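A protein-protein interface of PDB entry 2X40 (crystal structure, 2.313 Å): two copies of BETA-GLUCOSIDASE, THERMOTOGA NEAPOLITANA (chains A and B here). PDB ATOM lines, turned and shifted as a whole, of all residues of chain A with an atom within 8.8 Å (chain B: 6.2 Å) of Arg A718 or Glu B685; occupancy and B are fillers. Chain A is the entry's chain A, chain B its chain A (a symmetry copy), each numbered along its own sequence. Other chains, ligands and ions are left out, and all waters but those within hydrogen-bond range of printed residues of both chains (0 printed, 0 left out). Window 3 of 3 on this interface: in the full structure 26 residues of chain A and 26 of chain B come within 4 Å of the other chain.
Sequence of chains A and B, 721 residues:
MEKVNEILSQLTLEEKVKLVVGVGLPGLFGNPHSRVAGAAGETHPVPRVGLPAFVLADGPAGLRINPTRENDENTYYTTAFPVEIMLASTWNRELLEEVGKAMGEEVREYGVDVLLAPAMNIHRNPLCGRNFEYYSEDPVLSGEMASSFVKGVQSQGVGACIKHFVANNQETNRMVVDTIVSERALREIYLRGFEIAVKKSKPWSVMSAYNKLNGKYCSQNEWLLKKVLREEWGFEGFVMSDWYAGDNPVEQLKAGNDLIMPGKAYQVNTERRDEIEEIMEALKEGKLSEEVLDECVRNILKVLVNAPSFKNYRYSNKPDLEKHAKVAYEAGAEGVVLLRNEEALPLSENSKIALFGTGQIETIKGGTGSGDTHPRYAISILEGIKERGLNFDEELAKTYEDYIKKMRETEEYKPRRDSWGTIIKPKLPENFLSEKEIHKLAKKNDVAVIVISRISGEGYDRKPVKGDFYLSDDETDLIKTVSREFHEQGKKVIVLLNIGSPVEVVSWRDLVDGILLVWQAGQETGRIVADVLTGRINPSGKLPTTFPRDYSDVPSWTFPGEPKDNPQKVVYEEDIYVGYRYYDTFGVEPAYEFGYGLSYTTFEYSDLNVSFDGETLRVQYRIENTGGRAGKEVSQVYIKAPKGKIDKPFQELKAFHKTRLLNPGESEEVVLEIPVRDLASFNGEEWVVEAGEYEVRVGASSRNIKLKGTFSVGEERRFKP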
ATOM      1  N   GLY A 644       1.834  32.296   0.262  1.00  0.00           N
ATOM      2  CA  GLY A 644       2.259  31.139  -0.509  1.00  0.00           C
ATOM      3  C   GLY A 644       3.413  30.343   0.088  1.00  0.00           C
ATOM      4  O   GLY A 644       3.331  29.849   1.220  1.00  0.00           O
ATOM      5  N   LYS A 645       4.498  30.229  -0.677  1.00  0.00           N
ATOM      6  CA  LYS A 645       5.599  29.327  -0.349  1.00  0.00           C
ATOM      7  C   LYS A 645       6.663  29.985   0.510  1.00  0.00           C
ATOM      8  O   LYS A 645       7.102  29.428   1.513  1.00  0.00           O
ATOM      9  CB  LYS A 645       6.272  28.813  -1.624  1.00  0.00           C
ATOM     10  CG  LYS A 645       5.329  28.422  -2.747  1.00  0.00           C
ATOM     11  CD  LYS A 645       5.012  26.947  -2.716  1.00  0.00           C
ATOM     12  CE  LYS A 645       4.648  26.441  -4.102  1.00  0.00           C
ATOM     13  NZ  LYS A 645       5.806  26.526  -5.033  1.00  0.00           N
ATOM     14  N   ILE A 646       7.090  31.170   0.101  1.00  0.00           N
ATOM     15  CA  ILE A 646       8.247  31.797   0.711  1.00  0.00           C
ATOM     16  C   ILE A 646       7.874  33.137   1.323  1.00  0.00           C
ATOM     17  O   ILE A 646       6.891  33.755   0.919  1.00  0.00           O
ATOM     18  CB  ILE A 646       9.365  31.984  -0.330  1.00  0.00           C
ATOM     19  CG1 ILE A 646      10.671  32.396   0.349  1.00  0.00           C
ATOM     20  CG2 ILE A 646       8.936  32.991  -1.409  1.00  0.00           C
ATOM     21  CD1 ILE A 646      11.873  32.369  -0.574  1.00  0.00           C
ATOM     22  N   VAL A 676       4.330  40.203 -16.036  1.00  0.00           N
ATOM     23  CA  VAL A 676       4.173  39.192 -14.987  1.00  0.00           C
ATOM     24  C   VAL A 676       5.499  38.825 -14.296  1.00  0.00           C
ATOM     25  O   VAL A 676       5.513  38.471 -13.115  1.00  0.00           O
ATOM     26  CB  VAL A 676       3.421  37.930 -15.506  1.00  0.00           C
ATOM     27  CG1 VAL A 676       4.065  37.387 -16.783  1.00  0.00           C
ATOM     28  CG2 VAL A 676       3.323  36.853 -14.415  1.00  0.00           C
ATOM     29  N   ARG A 677       6.604  38.939 -15.031  1.00  0.00           N
ATOM     30  CA  ARG A 677       7.938  38.658 -14.498  1.00  0.00           C
ATOM     31  C   ARG A 677       8.342  39.606 -13.354  1.00  0.00           C
ATOM     32  O   ARG A 677       9.202  39.273 -12.530  1.00  0.00           O
ATOM     33  CB  ARG A 677       8.968  38.705 -15.634  1.00  0.00           C
ATOM     34  CG  ARG A 677      10.411  38.419 -15.238  1.00  0.00           C
ATOM     35  CD  ARG A 677      11.294  38.263 -16.478  1.00  0.00           C
ATOM     36  NE  ARG A 677      10.947  37.065 -17.247  1.00  0.00           N
ATOM     37  CZ  ARG A 677      11.342  36.823 -18.496  1.00  0.00           C
ATOM     38  NH1 ARG A 677      12.100  37.701 -19.139  1.00  0.00           N
ATOM     39  NH2 ARG A 677      10.971  35.704 -19.107  1.00  0.00           N
ATOM     40  N   ALA A 680       7.609  38.576  -9.523  1.00  0.00           N
ATOM     41  CA  ALA A 680       8.345  37.434  -8.980  1.00  0.00           C
ATOM     42  C   ALA A 680       9.110  37.726  -7.691  1.00  0.00           C
ATOM     43  O   ALA A 680       9.420  38.876  -7.385  1.00  0.00           O
ATOM     44  CB  ALA A 680       9.298  36.884 -10.030  1.00  0.00           C
ATOM     45  N   SER A 681       9.398  36.663  -6.940  1.00  0.00           N
ATOM     46  CA  SER A 681      10.353  36.709  -5.833  1.00  0.00           C
ATOM     47  C   SER A 681      11.452  35.702  -6.119  1.00  0.00           C
ATOM     48  O   SER A 681      11.208  34.677  -6.754  1.00  0.00           O
ATOM     49  CB  SER A 681       9.688  36.346  -4.504  1.00  0.00           C
ATOM     50  OG  SER A 681       8.832  37.376  -4.056  1.00  0.00           O
ATOM     51  N   PHE A 682      12.659  35.987  -5.648  1.00  0.00           N
ATOM     52  CA  PHE A 682      13.778  35.079  -5.852  1.00  0.00           C
ATOM     53  C   PHE A 682      13.939  34.121  -4.666  1.00  0.00           C
ATOM     54  O   PHE A 682      14.068  34.553  -3.520  1.00  0.00           O
ATOM     55  CB  PHE A 682      15.060  35.871  -6.065  1.00  0.00           C
ATOM     56  CG  PHE A 682      16.183  35.052  -6.618  1.00  0.00           C
ATOM     57  CD1 PHE A 682      17.239  34.669  -5.811  1.00  0.00           C
ATOM     58  CD2 PHE A 682      16.172  34.649  -7.949  1.00  0.00           C
ATOM     59  CE1 PHE A 682      18.272  33.908  -6.320  1.00  0.00           C
ATOM     60  CE2 PHE A 682      17.201  33.888  -8.470  1.00  0.00           C
ATOM     61  CZ  PHE A 682      18.255  33.514  -7.655  1.00  0.00           C
ATOM     62  N   ASN A 683      13.935  32.820  -4.942  1.00  0.00           N
ATOM     63  CA  ASN A 683      13.995  31.834  -3.872  1.00  0.00           C
ATOM     64  C   ASN A 683      15.391  31.256  -3.639  1.00  0.00           C
ATOM     65  O   ASN A 683      15.547  30.253  -2.948  1.00  0.00           O
ATOM     66  CB  ASN A 683      12.979  30.715  -4.118  1.00  0.00           C
ATOM     67  CG  ASN A 683      13.415  29.752  -5.211  1.00  0.00           C
ATOM     68  OD1 ASN A 683      14.438  29.957  -5.869  1.00  0.00           O
ATOM     69  ND2 ASN A 683      12.639  28.685  -5.402  1.00  0.00           N
ATOM     70  N   GLY A 684      16.406  31.895  -4.215  1.00  0.00           N
ATOM     71  CA  GLY A 684      17.774  31.427  -4.077  1.00  0.00           C
ATOM     72  C   GLY A 684      18.310  30.794  -5.347  1.00  0.00           C
ATOM     73  O   GLY A 684      19.518  30.771  -5.583  1.00  0.00           O
ATOM     74  N   GLU A 685      17.406  30.280  -6.174  1.00  0.00           N
ATOM     75  CA  GLU A 685      17.796  29.656  -7.428  1.00  0.00           C
ATOM     76  C   GLU A 685      17.041  30.253  -8.600  1.00  0.00           C
ATOM     77  O   GLU A 685      17.624  30.535  -9.647  1.00  0.00           O
ATOM     78  CB  GLU A 685      17.556  28.143  -7.382  1.00  0.00           C
ATOM     79  CG  GLU A 685      18.743  27.342  -6.879  1.00  0.00           C
ATOM     80  CD  GLU A 685      18.466  26.655  -5.557  1.00  0.00           C
ATOM     81  OE1 GLU A 685      19.434  26.208  -4.906  1.00  0.00           O
ATOM     82  OE2 GLU A 685      17.282  26.562  -5.171  1.00  0.00           O
ATOM     83  N   GLU A 686      15.740  30.437  -8.420  1.00  0.00           N
ATOM     84  CA  GLU A 686      14.884  30.888  -9.507  1.00  0.00           C
ATOM     85  C   GLU A 686      13.980  32.039  -9.097  1.00  0.00           C
ATOM     86  O   GLU A 686      13.648  32.200  -7.925  1.00  0.00           O
ATOM     87  CB  GLU A 686      14.005  29.736  -9.996  1.00  0.00           C
ATOM     88  CG  GLU A 686      14.748  28.458 -10.296  1.00  0.00           C
ATOM     89  CD  GLU A 686      13.841  27.405 -10.895  1.00  0.00           C
ATOM     90  OE1 GLU A 686      14.337  26.310 -11.238  1.00  0.00           O
ATOM     91  OE2 GLU A 686      12.630  27.680 -11.027  1.00  0.00           O
ATOM     92  N   TRP A 687      13.583  32.836 -10.078  1.00  0.00           N
ATOM     93  CA  TRP A 687      12.504  33.786  -9.892  1.00  0.00           C
ATOM     94  C   TRP A 687      11.204  33.008  -9.962  1.00  0.00           C
ATOM     95  O   TRP A 687      11.005  32.208 -10.874  1.00  0.00           O
ATOM     96  CB  TRP A 687      12.529  34.850 -10.994  1.00  0.00           C
ATOM     97  CG  TRP A 687      13.624  35.862 -10.814  1.00  0.00           C
ATOM     98  CD1 TRP A 687      14.842  35.874 -11.429  1.00  0.00           C
ATOM     99  CD2 TRP A 687      13.602  37.003  -9.948  1.00  0.00           C
ATOM    100  NE1 TRP A 687      15.576  36.953 -11.005  1.00  0.00           N
ATOM    101  CE2 TRP A 687      14.838  37.663 -10.093  1.00  0.00           C
ATOM    102  CE3 TRP A 687      12.653  37.534  -9.068  1.00  0.00           C
ATOM    103  CZ2 TRP A 687      15.152  38.824  -9.392  1.00  0.00           C
ATOM    104  CZ3 TRP A 687      12.967  38.691  -8.376  1.00  0.00           C
ATOM    105  CH2 TRP A 687      14.203  39.322  -8.541  1.00  0.00           C
ATOM    106  N   VAL A 688      10.324  33.230  -8.998  1.00  0.00           N
ATOM    107  CA  VAL A 688       9.040  32.549  -8.997  1.00  0.00           C
ATOM    108  C   VAL A 688       7.890  33.539  -8.883  1.00  0.00           C
ATOM    109  O   VAL A 688       7.879  34.410  -8.009  1.00  0.00           O
ATOM    110  CB  VAL A 688       8.935  31.520  -7.837  1.00  0.00           C
ATOM    111  CG1 VAL A 688       7.570  30.836  -7.840  1.00  0.00           C
ATOM    112  CG2 VAL A 688      10.054  30.488  -7.926  1.00  0.00           C
ATOM    113  N   VAL A 689       6.930  33.409  -9.788  1.00  0.00           N
ATOM    114  CA  VAL A 689       5.658  34.092  -9.638  1.00  0.00           C
ATOM    115  C   VAL A 689       4.655  33.058  -9.160  1.00  0.00           C
ATOM    116  O   VAL A 689       4.133  32.267  -9.954  1.00  0.00           O
ATOM    117  CB  VAL A 689       5.164  34.701 -10.958  1.00  0.00           C
ATOM    118  CG1 VAL A 689       3.772  35.286 -10.767  1.00  0.00           C
ATOM    119  CG2 VAL A 689       6.141  35.764 -11.452  1.00  0.00           C
ATOM    120  N   GLU A 690       4.412  33.054  -7.855  1.00  0.00           N
ATOM    121  CA  GLU A 690       3.527  32.077  -7.239  1.00  0.00           C
ATOM    122  C   GLU A 690       2.080  32.297  -7.647  1.00  0.00           C
ATOM    123  O   GLU A 690       1.638  33.430  -7.833  1.00  0.00           O
ATOM    124  CB  GLU A 690       3.642  32.142  -5.720  1.00  0.00           C
ATOM    125  CG  GLU A 690       5.021  31.806  -5.195  1.00  0.00           C
ATOM    126  CD  GLU A 690       5.122  31.964  -3.691  1.00  0.00           C
ATOM    127  OE1 GLU A 690       6.256  32.087  -3.183  1.00  0.00           O
ATOM    128  OE2 GLU A 690       4.066  31.975  -3.023  1.00  0.00           O
ATOM    129  N   GLU A 715      -1.601  29.835 -12.895  1.00  0.00           N
ATOM    130  CA  GLU A 715      -0.476  28.914 -12.921  1.00  0.00           C
ATOM    131  C   GLU A 715       0.814  29.612 -12.520  1.00  0.00           C
ATOM    132  O   GLU A 715       1.132  30.699 -13.007  1.00  0.00           O
ATOM    133  CB  GLU A 715      -0.329  28.283 -14.304  1.00  0.00           C
ATOM    134  CG  GLU A 715      -0.545  26.780 -14.314  1.00  0.00           C
ATOM    135  CD  GLU A 715      -1.320  26.312 -15.531  1.00  0.00           C
ATOM    136  OE1 GLU A 715      -1.597  27.150 -16.418  1.00  0.00           O
ATOM    137  OE2 GLU A 715      -1.658  25.110 -15.595  1.00  0.00           O
ATOM    138  N   GLU A 716       1.545  28.977 -11.615  1.00  0.00           N
ATOM    139  CA  GLU A 716       2.847  29.461 -11.192  1.00  0.00           C
ATOM    140  C   GLU A 716       3.765  29.631 -12.400  1.00  0.00           C
ATOM    141  O   GLU A 716       3.618  28.939 -13.408  1.00  0.00           O
ATOM    142  CB  GLU A 716       3.452  28.478 -10.194  1.00  0.00           C
ATOM    143  CG  GLU A 716       4.879  28.764  -9.796  1.00  0.00           C
ATOM    144  CD  GLU A 716       5.372  27.807  -8.729  1.00  0.00           C
ATOM    145  OE1 GLU A 716       5.101  28.050  -7.530  1.00  0.00           O
ATOM    146  OE2 GLU A 716       6.024  26.804  -9.092  1.00  0.00           O
ATOM    147  N   ARG A 717       4.705  30.562 -12.294  1.00  0.00           N
ATOM    148  CA  ARG A 717       5.660  30.824 -13.361  1.00  0.00           C
ATOM    149  C   ARG A 717       7.063  30.861 -12.770  1.00  0.00           C
ATOM    150  O   ARG A 717       7.262  31.392 -11.680  1.00  0.00           O
ATOM    151  CB  ARG A 717       5.339  32.161 -14.022  1.00  0.00           C
ATOM    152  CG  ARG A 717       3.871  32.342 -14.391  1.00  0.00           C
ATOM    153  CD  ARG A 717       3.571  31.716 -15.734  1.00  0.00           C
ATOM    154  NE  ARG A 717       4.661  31.959 -16.673  1.00  0.00           N
ATOM    155  CZ  ARG A 717       4.742  33.019 -17.469  1.00  0.00           C
ATOM    156  NH1 ARG A 717       3.787  33.940 -17.450  1.00  0.00           N
ATOM    157  NH2 ARG A 717       5.775  33.154 -18.289  1.00  0.00           N
ATOM    158  N   ARG A 718       8.032  30.296 -13.484  1.00  0.00           N
ATOM    159  CA  ARG A 718       9.400  30.218 -12.980  1.00  0.00           C
ATOM    160  C   ARG A 718      10.408  30.718 -14.011  1.00  0.00           C
ATOM    161  O   ARG A 718      10.217  30.522 -15.206  1.00  0.00           O
ATOM    162  CB  ARG A 718       9.728  28.779 -12.572  1.00  0.00           C
ATOM    163  CG  ARG A 718       8.749  28.180 -11.569  1.00  0.00           C
ATOM    164  CD  ARG A 718       9.137  26.754 -11.162  1.00  0.00           C
ATOM    165  NE  ARG A 718      10.339  26.716 -10.330  1.00  0.00           N
ATOM    166  CZ  ARG A 718      10.336  26.768  -9.001  1.00  0.00           C
ATOM    167  NH1 ARG A 718       9.189  26.859  -8.341  1.00  0.00           N
ATOM    168  NH2 ARG A 718      11.480  26.730  -8.328  1.00  0.00           N
ATOM    169  N   PHE A 719      11.475  31.364 -13.546  1.00  0.00           N
ATOM    170  CA  PHE A 719      12.519  31.884 -14.434  1.00  0.00           C
ATOM    171  C   PHE A 719      13.912  31.681 -13.845  1.00  0.00           C
ATOM    172  O   PHE A 719      14.290  32.352 -12.887  1.00  0.00           O
ATOM    173  CB  PHE A 719      12.330  33.382 -14.697  1.00  0.00           C
ATOM    174  CG  PHE A 719      10.933  33.769 -15.074  1.00  0.00           C
ATOM    175  CD1 PHE A 719      10.460  33.546 -16.359  1.00  0.00           C
ATOM    176  CD2 PHE A 719      10.103  34.388 -14.158  1.00  0.00           C
ATOM    177  CE1 PHE A 719       9.172  33.920 -16.715  1.00  0.00           C
ATOM    178  CE2 PHE A 719       8.816  34.761 -14.505  1.00  0.00           C
ATOM    179  CZ  PHE A 719       8.349  34.529 -15.786  1.00  0.00           C
ATOM    180  N   LYS A 720      14.681  30.770 -14.427  1.00  0.00           N
ATOM    181  CA  LYS A 720      16.061  30.566 -14.007  1.00  0.00           C
ATOM    182  C   LYS A 720      16.983  31.388 -14.901  1.00  0.00           C
ATOM    183  O   LYS A 720      17.030  31.170 -16.112  1.00  0.00           O
ATOM    184  CB  LYS A 720      16.424  29.080 -14.078  1.00  0.00           C
ATOM    185  CG  LYS A 720      17.676  28.699 -13.301  1.00  0.00           C
ATOM    186  CD  LYS A 720      17.465  27.402 -12.527  1.00  0.00           C
ATOM    187  CE  LYS A 720      17.016  26.270 -13.442  1.00  0.00           C
ATOM    188  NZ  LYS A 720      16.726  25.022 -12.683  1.00  0.00           N
ATOM    189  N   PRO A 721      17.718  32.343 -14.309  1.00  0.00           N
ATOM    190  CA  PRO A 721      18.558  33.264 -15.088  1.00  0.00           C
ATOM    191  C   PRO A 721      19.720  32.553 -15.786  1.00  0.00           C
ATOM    192  O   PRO A 721      19.686  32.358 -17.006  1.00  0.00           O
ATOM    193  CB  PRO A 721      19.087  34.241 -14.028  1.00  0.00           C
ATOM    194  CG  PRO A 721      18.255  34.011 -12.807  1.00  0.00           C
ATOM    195  CD  PRO A 721      17.827  32.587 -12.863  1.00  0.00           C
ATOM    196  N   GLU B 183       4.390  28.827   3.483  1.00  0.00           N
ATOM    197  CA  GLU B 183       4.852  27.475   3.714  1.00  0.00           C
ATOM    198  C   GLU B 183       6.216  27.466   4.422  1.00  0.00           C
ATOM    199  O   GLU B 183       6.483  26.581   5.236  1.00  0.00           O
ATOM    200  CB  GLU B 183       4.897  26.675   2.415  1.00  0.00           C
ATOM    201  CG  GLU B 183       5.283  25.230   2.647  1.00  0.00           C
ATOM    202  CD  GLU B 183       4.973  24.327   1.479  1.00  0.00           C
ATOM    203  OE1 GLU B 183       5.444  23.171   1.514  1.00  0.00           O
ATOM    204  OE2 GLU B 183       4.266  24.762   0.538  1.00  0.00           O
ATOM    205  N   ARG B 187       7.013  25.448   7.911  1.00  0.00           N
ATOM    206  CA  ARG B 187       7.999  24.392   8.046  1.00  0.00           C
ATOM    207  C   ARG B 187       9.171  24.722   8.970  1.00  0.00           C
ATOM    208  O   ARG B 187       9.729  23.832   9.607  1.00  0.00           O
ATOM    209  CB  ARG B 187       8.480  23.936   6.669  1.00  0.00           C
ATOM    210  CG  ARG B 187       7.385  23.218   5.892  1.00  0.00           C
ATOM    211  CD  ARG B 187       7.938  22.485   4.691  1.00  0.00           C
ATOM    212  NE  ARG B 187       6.875  21.937   3.849  1.00  0.00           N
ATOM    213  CZ  ARG B 187       6.328  20.737   4.018  1.00  0.00           C
ATOM    214  NH1 ARG B 187       6.741  19.955   5.004  1.00  0.00           N
ATOM    215  NH2 ARG B 187       5.372  20.319   3.200  1.00  0.00           N
ATOM    216  N   PHE B 682      14.223  26.287   4.555  1.00  0.00           N
ATOM    217  CA  PHE B 682      13.236  25.938   3.545  1.00  0.00           C
ATOM    218  C   PHE B 682      13.057  27.072   2.529  1.00  0.00           C
ATOM    219  O   PHE B 682      12.763  28.209   2.900  1.00  0.00           O
ATOM    220  CB  PHE B 682      11.905  25.609   4.206  1.00  0.00           C
ATOM    221  CG  PHE B 682      10.941  24.916   3.296  1.00  0.00           C
ATOM    222  CD1 PHE B 682       9.854  25.593   2.774  1.00  0.00           C
ATOM    223  CD2 PHE B 682      11.135  23.583   2.949  1.00  0.00           C
ATOM    224  CE1 PHE B 682       8.968  24.954   1.930  1.00  0.00           C
ATOM    225  CE2 PHE B 682      10.253  22.933   2.106  1.00  0.00           C
ATOM    226  CZ  PHE B 682       9.168  23.618   1.592  1.00  0.00           C
ATOM    227  N   ASN B 683      13.230  26.762   1.247  1.00  0.00           N
ATOM    228  CA  ASN B 683      13.165  27.792   0.219  1.00  0.00           C
ATOM    229  C   ASN B 683      11.823  27.856  -0.510  1.00  0.00           C
ATOM    230  O   ASN B 683      11.705  28.498  -1.550  1.00  0.00           O
ATOM    231  CB  ASN B 683      14.316  27.626  -0.777  1.00  0.00           C
ATOM    232  CG  ASN B 683      14.103  26.465  -1.736  1.00  0.00           C
ATOM    233  OD1 ASN B 683      13.138  25.707  -1.614  1.00  0.00           O
ATOM    234  ND2 ASN B 683      15.006  26.329  -2.709  1.00  0.00           N
ATOM    235  N   GLY B 684      10.811  27.192   0.042  1.00  0.00           N
ATOM    236  CA  GLY B 684       9.495  27.168  -0.571  1.00  0.00           C
ATOM    237  C   GLY B 684       9.166  25.830  -1.207  1.00  0.00           C
ATOM    238  O   GLY B 684       7.999  25.464  -1.346  1.00  0.00           O
ATOM    239  N   GLU B 685      10.201  25.092  -1.591  1.00  0.00           N
ATOM    240  CA  GLU B 685      10.014  23.786  -2.202  1.00  0.00           C
ATOM    241  C   GLU B 685      10.818  22.720  -1.485  1.00  0.00           C
ATOM    242  O   GLU B 685      10.321  21.624  -1.224  1.00  0.00           O
ATOM    243  CB  GLU B 685      10.409  23.815  -3.683  1.00  0.00           C
ATOM    244  CG  GLU B 685       9.270  24.165  -4.623  1.00  0.00           C
ATOM    245  CD  GLU B 685       9.480  25.489  -5.329  1.00  0.00           C
ATOM    246  OE1 GLU B 685       8.504  26.020  -5.899  1.00  0.00           O
ATOM    247  OE2 GLU B 685      10.621  25.999  -5.312  1.00  0.00           O
ATOM    248  N   GLU B 686      12.066  23.044  -1.173  1.00  0.00           N
ATOM    249  CA  GLU B 686      12.977  22.069  -0.593  1.00  0.00           C
ATOM    250  C   GLU B 686      13.703  22.606   0.630  1.00  0.00           C
ATOM    251  O   GLU B 686      13.892  23.812   0.779  1.00  0.00           O
ATOM    252  CB  GLU B 686      14.021  21.646  -1.626  1.00  0.00           C
ATOM    253  CG  GLU B 686      13.456  21.232  -2.962  1.00  0.00           C
ATOM    254  CD  GLU B 686      14.529  20.705  -3.890  1.00  0.00           C
ATOM    255  OE1 GLU B 686      14.193  20.280  -5.017  1.00  0.00           O
ATOM    256  OE2 GLU B 686      15.711  20.713  -3.486  1.00  0.00           O
ATOM    257  N   TRP B 687      14.112  21.696   1.501  1.00  0.00           N
ATOM    258  CA  TRP B 687      15.057  22.024   2.551  1.00  0.00           C
ATOM    259  C   TRP B 687      16.433  22.073   1.916  1.00  0.00           C
ATOM    260  O   TRP B 687      16.812  21.167   1.178  1.00  0.00           O
ATOM    261  CB  TRP B 687      15.033  20.956   3.648  1.00  0.00           C
ATOM    262  CG  TRP B 687      13.822  21.045   4.533  1.00  0.00           C
ATOM    263  CD1 TRP B 687      12.680  20.302   4.442  1.00  0.00           C
ATOM    264  CD2 TRP B 687      13.630  21.940   5.635  1.00  0.00           C
ATOM    265  NE1 TRP B 687      11.794  20.675   5.421  1.00  0.00           N
ATOM    266  CE2 TRP B 687      12.352  21.680   6.167  1.00  0.00           C
ATOM    267  CE3 TRP B 687      14.419  22.931   6.228  1.00  0.00           C
ATOM    268  CZ2 TRP B 687      11.843  22.376   7.261  1.00  0.00           C
ATOM    269  CZ3 TRP B 687      13.911  23.618   7.318  1.00  0.00           C
ATOM    270  CH2 TRP B 687      12.638  23.337   7.821  1.00  0.00           C
ATOM    271  N   PHE B 719      16.717  18.437   0.394  1.00  0.00           N
ATOM    272  CA  PHE B 719      15.722  17.456   0.837  1.00  0.00           C
ATOM    273  C   PHE B 719      14.305  17.885   0.467  1.00  0.00           C
ATOM    274  O   PHE B 719      13.759  18.816   1.056  1.00  0.00           O
ATOM    275  CB  PHE B 719      15.775  17.257   2.356  1.00  0.00           C
ATOM    276  CG  PHE B 719      17.153  17.044   2.901  1.00  0.00           C
ATOM    277  CD1 PHE B 719      17.780  15.812   2.779  1.00  0.00           C
ATOM    278  CD2 PHE B 719      17.811  18.061   3.567  1.00  0.00           C
ATOM    279  CE1 PHE B 719      19.049  15.607   3.299  1.00  0.00           C
ATOM    280  CE2 PHE B 719      19.080  17.866   4.086  1.00  0.00           C
ATOM    281  CZ  PHE B 719      19.700  16.637   3.955  1.00  0.00           C
ATOM    282  N   LYS B 720      13.704  17.199  -0.496  1.00  0.00           N
ATOM    283  CA  LYS B 720      12.318  17.461  -0.859  1.00  0.00           C
ATOM    284  C   LYS B 720      11.411  16.496  -0.103  1.00  0.00           C
ATOM    285  O   LYS B 720      11.515  15.282  -0.278  1.00  0.00           O
ATOM    286  CB  LYS B 720      12.127  17.310  -2.371  1.00  0.00           C
ATOM    287  CG  LYS B 720      10.849  17.936  -2.911  1.00  0.00           C
ATOM    288  CD  LYS B 720      11.117  18.692  -4.209  1.00  0.00           C
ATOM    289  CE  LYS B 720      11.779  17.800  -5.250  1.00  0.00           C
ATOM    290  NZ  LYS B 720      12.121  18.550  -6.490  1.00  0.00           N
ATOM    291  N   PRO B 721      10.519  17.031   0.745  1.00  0.00           N
ATOM    292  CA  PRO B 721       9.671  16.193   1.604  1.00  0.00           C
ATOM    293  C   PRO B 721       8.672  15.354   0.803  1.00  0.00           C
ATOM    294  O   PRO B 721       8.854  14.139   0.661  1.00  0.00           O
ATOM    295  CB  PRO B 721       8.932  17.216   2.477  1.00  0.00           C
ATOM    296  CG  PRO B 721       9.651  18.513   2.288  1.00  0.00           C
ATOM    297  CD  PRO B 721      10.234  18.463   0.920  1.00  0.00           C
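The backbone NH (N) of Glu B183 is in hydrogen-bond range of the backbone carbonyl oxygen (O) of Gly A644 (2.7 Å). The backbone carbonyl oxygen (O) of Lys A645 is in hydrogen-bond range of the backbone NH (N) of Glu B183. NZ of Lys A645 lies within salt-bridge range of OE1 of Glu B685. ND2 of Asn A683 is in hydrogen-bond range of OE2 of Glu B685, 3.4 Å away. The side-chain carboxylate (OE2) of Glu A685 lies within hydrogen-bond range of the side-chain amide nitrogen (ND2) of Asn B683 (3.4 Å). The guanidinium group (NH1) of Arg A718 lies within salt-bridge range of the side-chain carboxylate (OE1) of Glu B685, at 2.7 Å.
NZ of Lys A645 is in salt-bridge range of OE1 of Glu A716 (3.0 Å). The side-chain amide oxygen (OD1) of Asn A683 is in hydrogen-bond range of the backbone NH (N) of Glu A686, 2.9 Å away. The guanidinium group (NH1) of Arg A718 is in salt-bridge range of the side-chain carboxylate (OE2) of Glu A716 (3.3 Å). N of Glu B685 is in hydrogen-bond range of OD1 of Asn B683, at 3.0 Å.
Gly B684 touches Lys A645 (O to CD, 3.6 Å). O of Asn B683 touches CD1 of Ile A646, at 3.996 Å. Asn A683 touches Asn B683 (O to CB, 3.6 Å).
Of the printed residues of chain B, Gly A644 touches Glu B183 (2.7 Å). Printed residues of chain B within 4 Å of Ile A646: Asn B683. Of the printed residues of chain B, Asn A683 touches Asn B683 (3.6 Å) and Glu B685 (3.4 Å). Of the printed residues of chain B, Glu A685 touches Asn B683. Of chain B, only Glu B685 (2.7 Å) comes within 4 Å of Arg A718. Of the printed residues of chain A, Glu B685 touches Lys A645 (2.9 Å), Asn A683 (3.4 Å) and Arg A718 (2.7 Å).
Of the 23 printed residues of chain A, 6 touch a printed residue of chain B. Printed residues of chain A that touch a printed residue of chain B: Gly A644, Lys A645, Ile A646, Asn A683, Glu A685 and Arg A718. Hydrophobic or aromatic side chains of chain A that line the printed part of chain B: Ile A646. Of the 11 printed residues of chain B, 4 touch a printed residue of chain A. Among the printed residues, 9 pairs touch across the chains. Among the printed residues, Asp or Glu carboxylates within 4 Å of a Lys or Arg side-chain nitrogen of the other chain: Lys A645 with Glu B685 and Arg A718 with Glu B685.
Asn B683 touches its own counterpart, Asn A683. Asn A683 touches Glu B685, and with the chains exchanged Glu A685 touches Asn B683. Positions printed for both chains: 682, 683, 684, 685, 686, 687, 719, 720 and 721. Of the 9 pairs that touch across the chains among the printed residues, 3 have their exchanged pair printed and touching as well.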
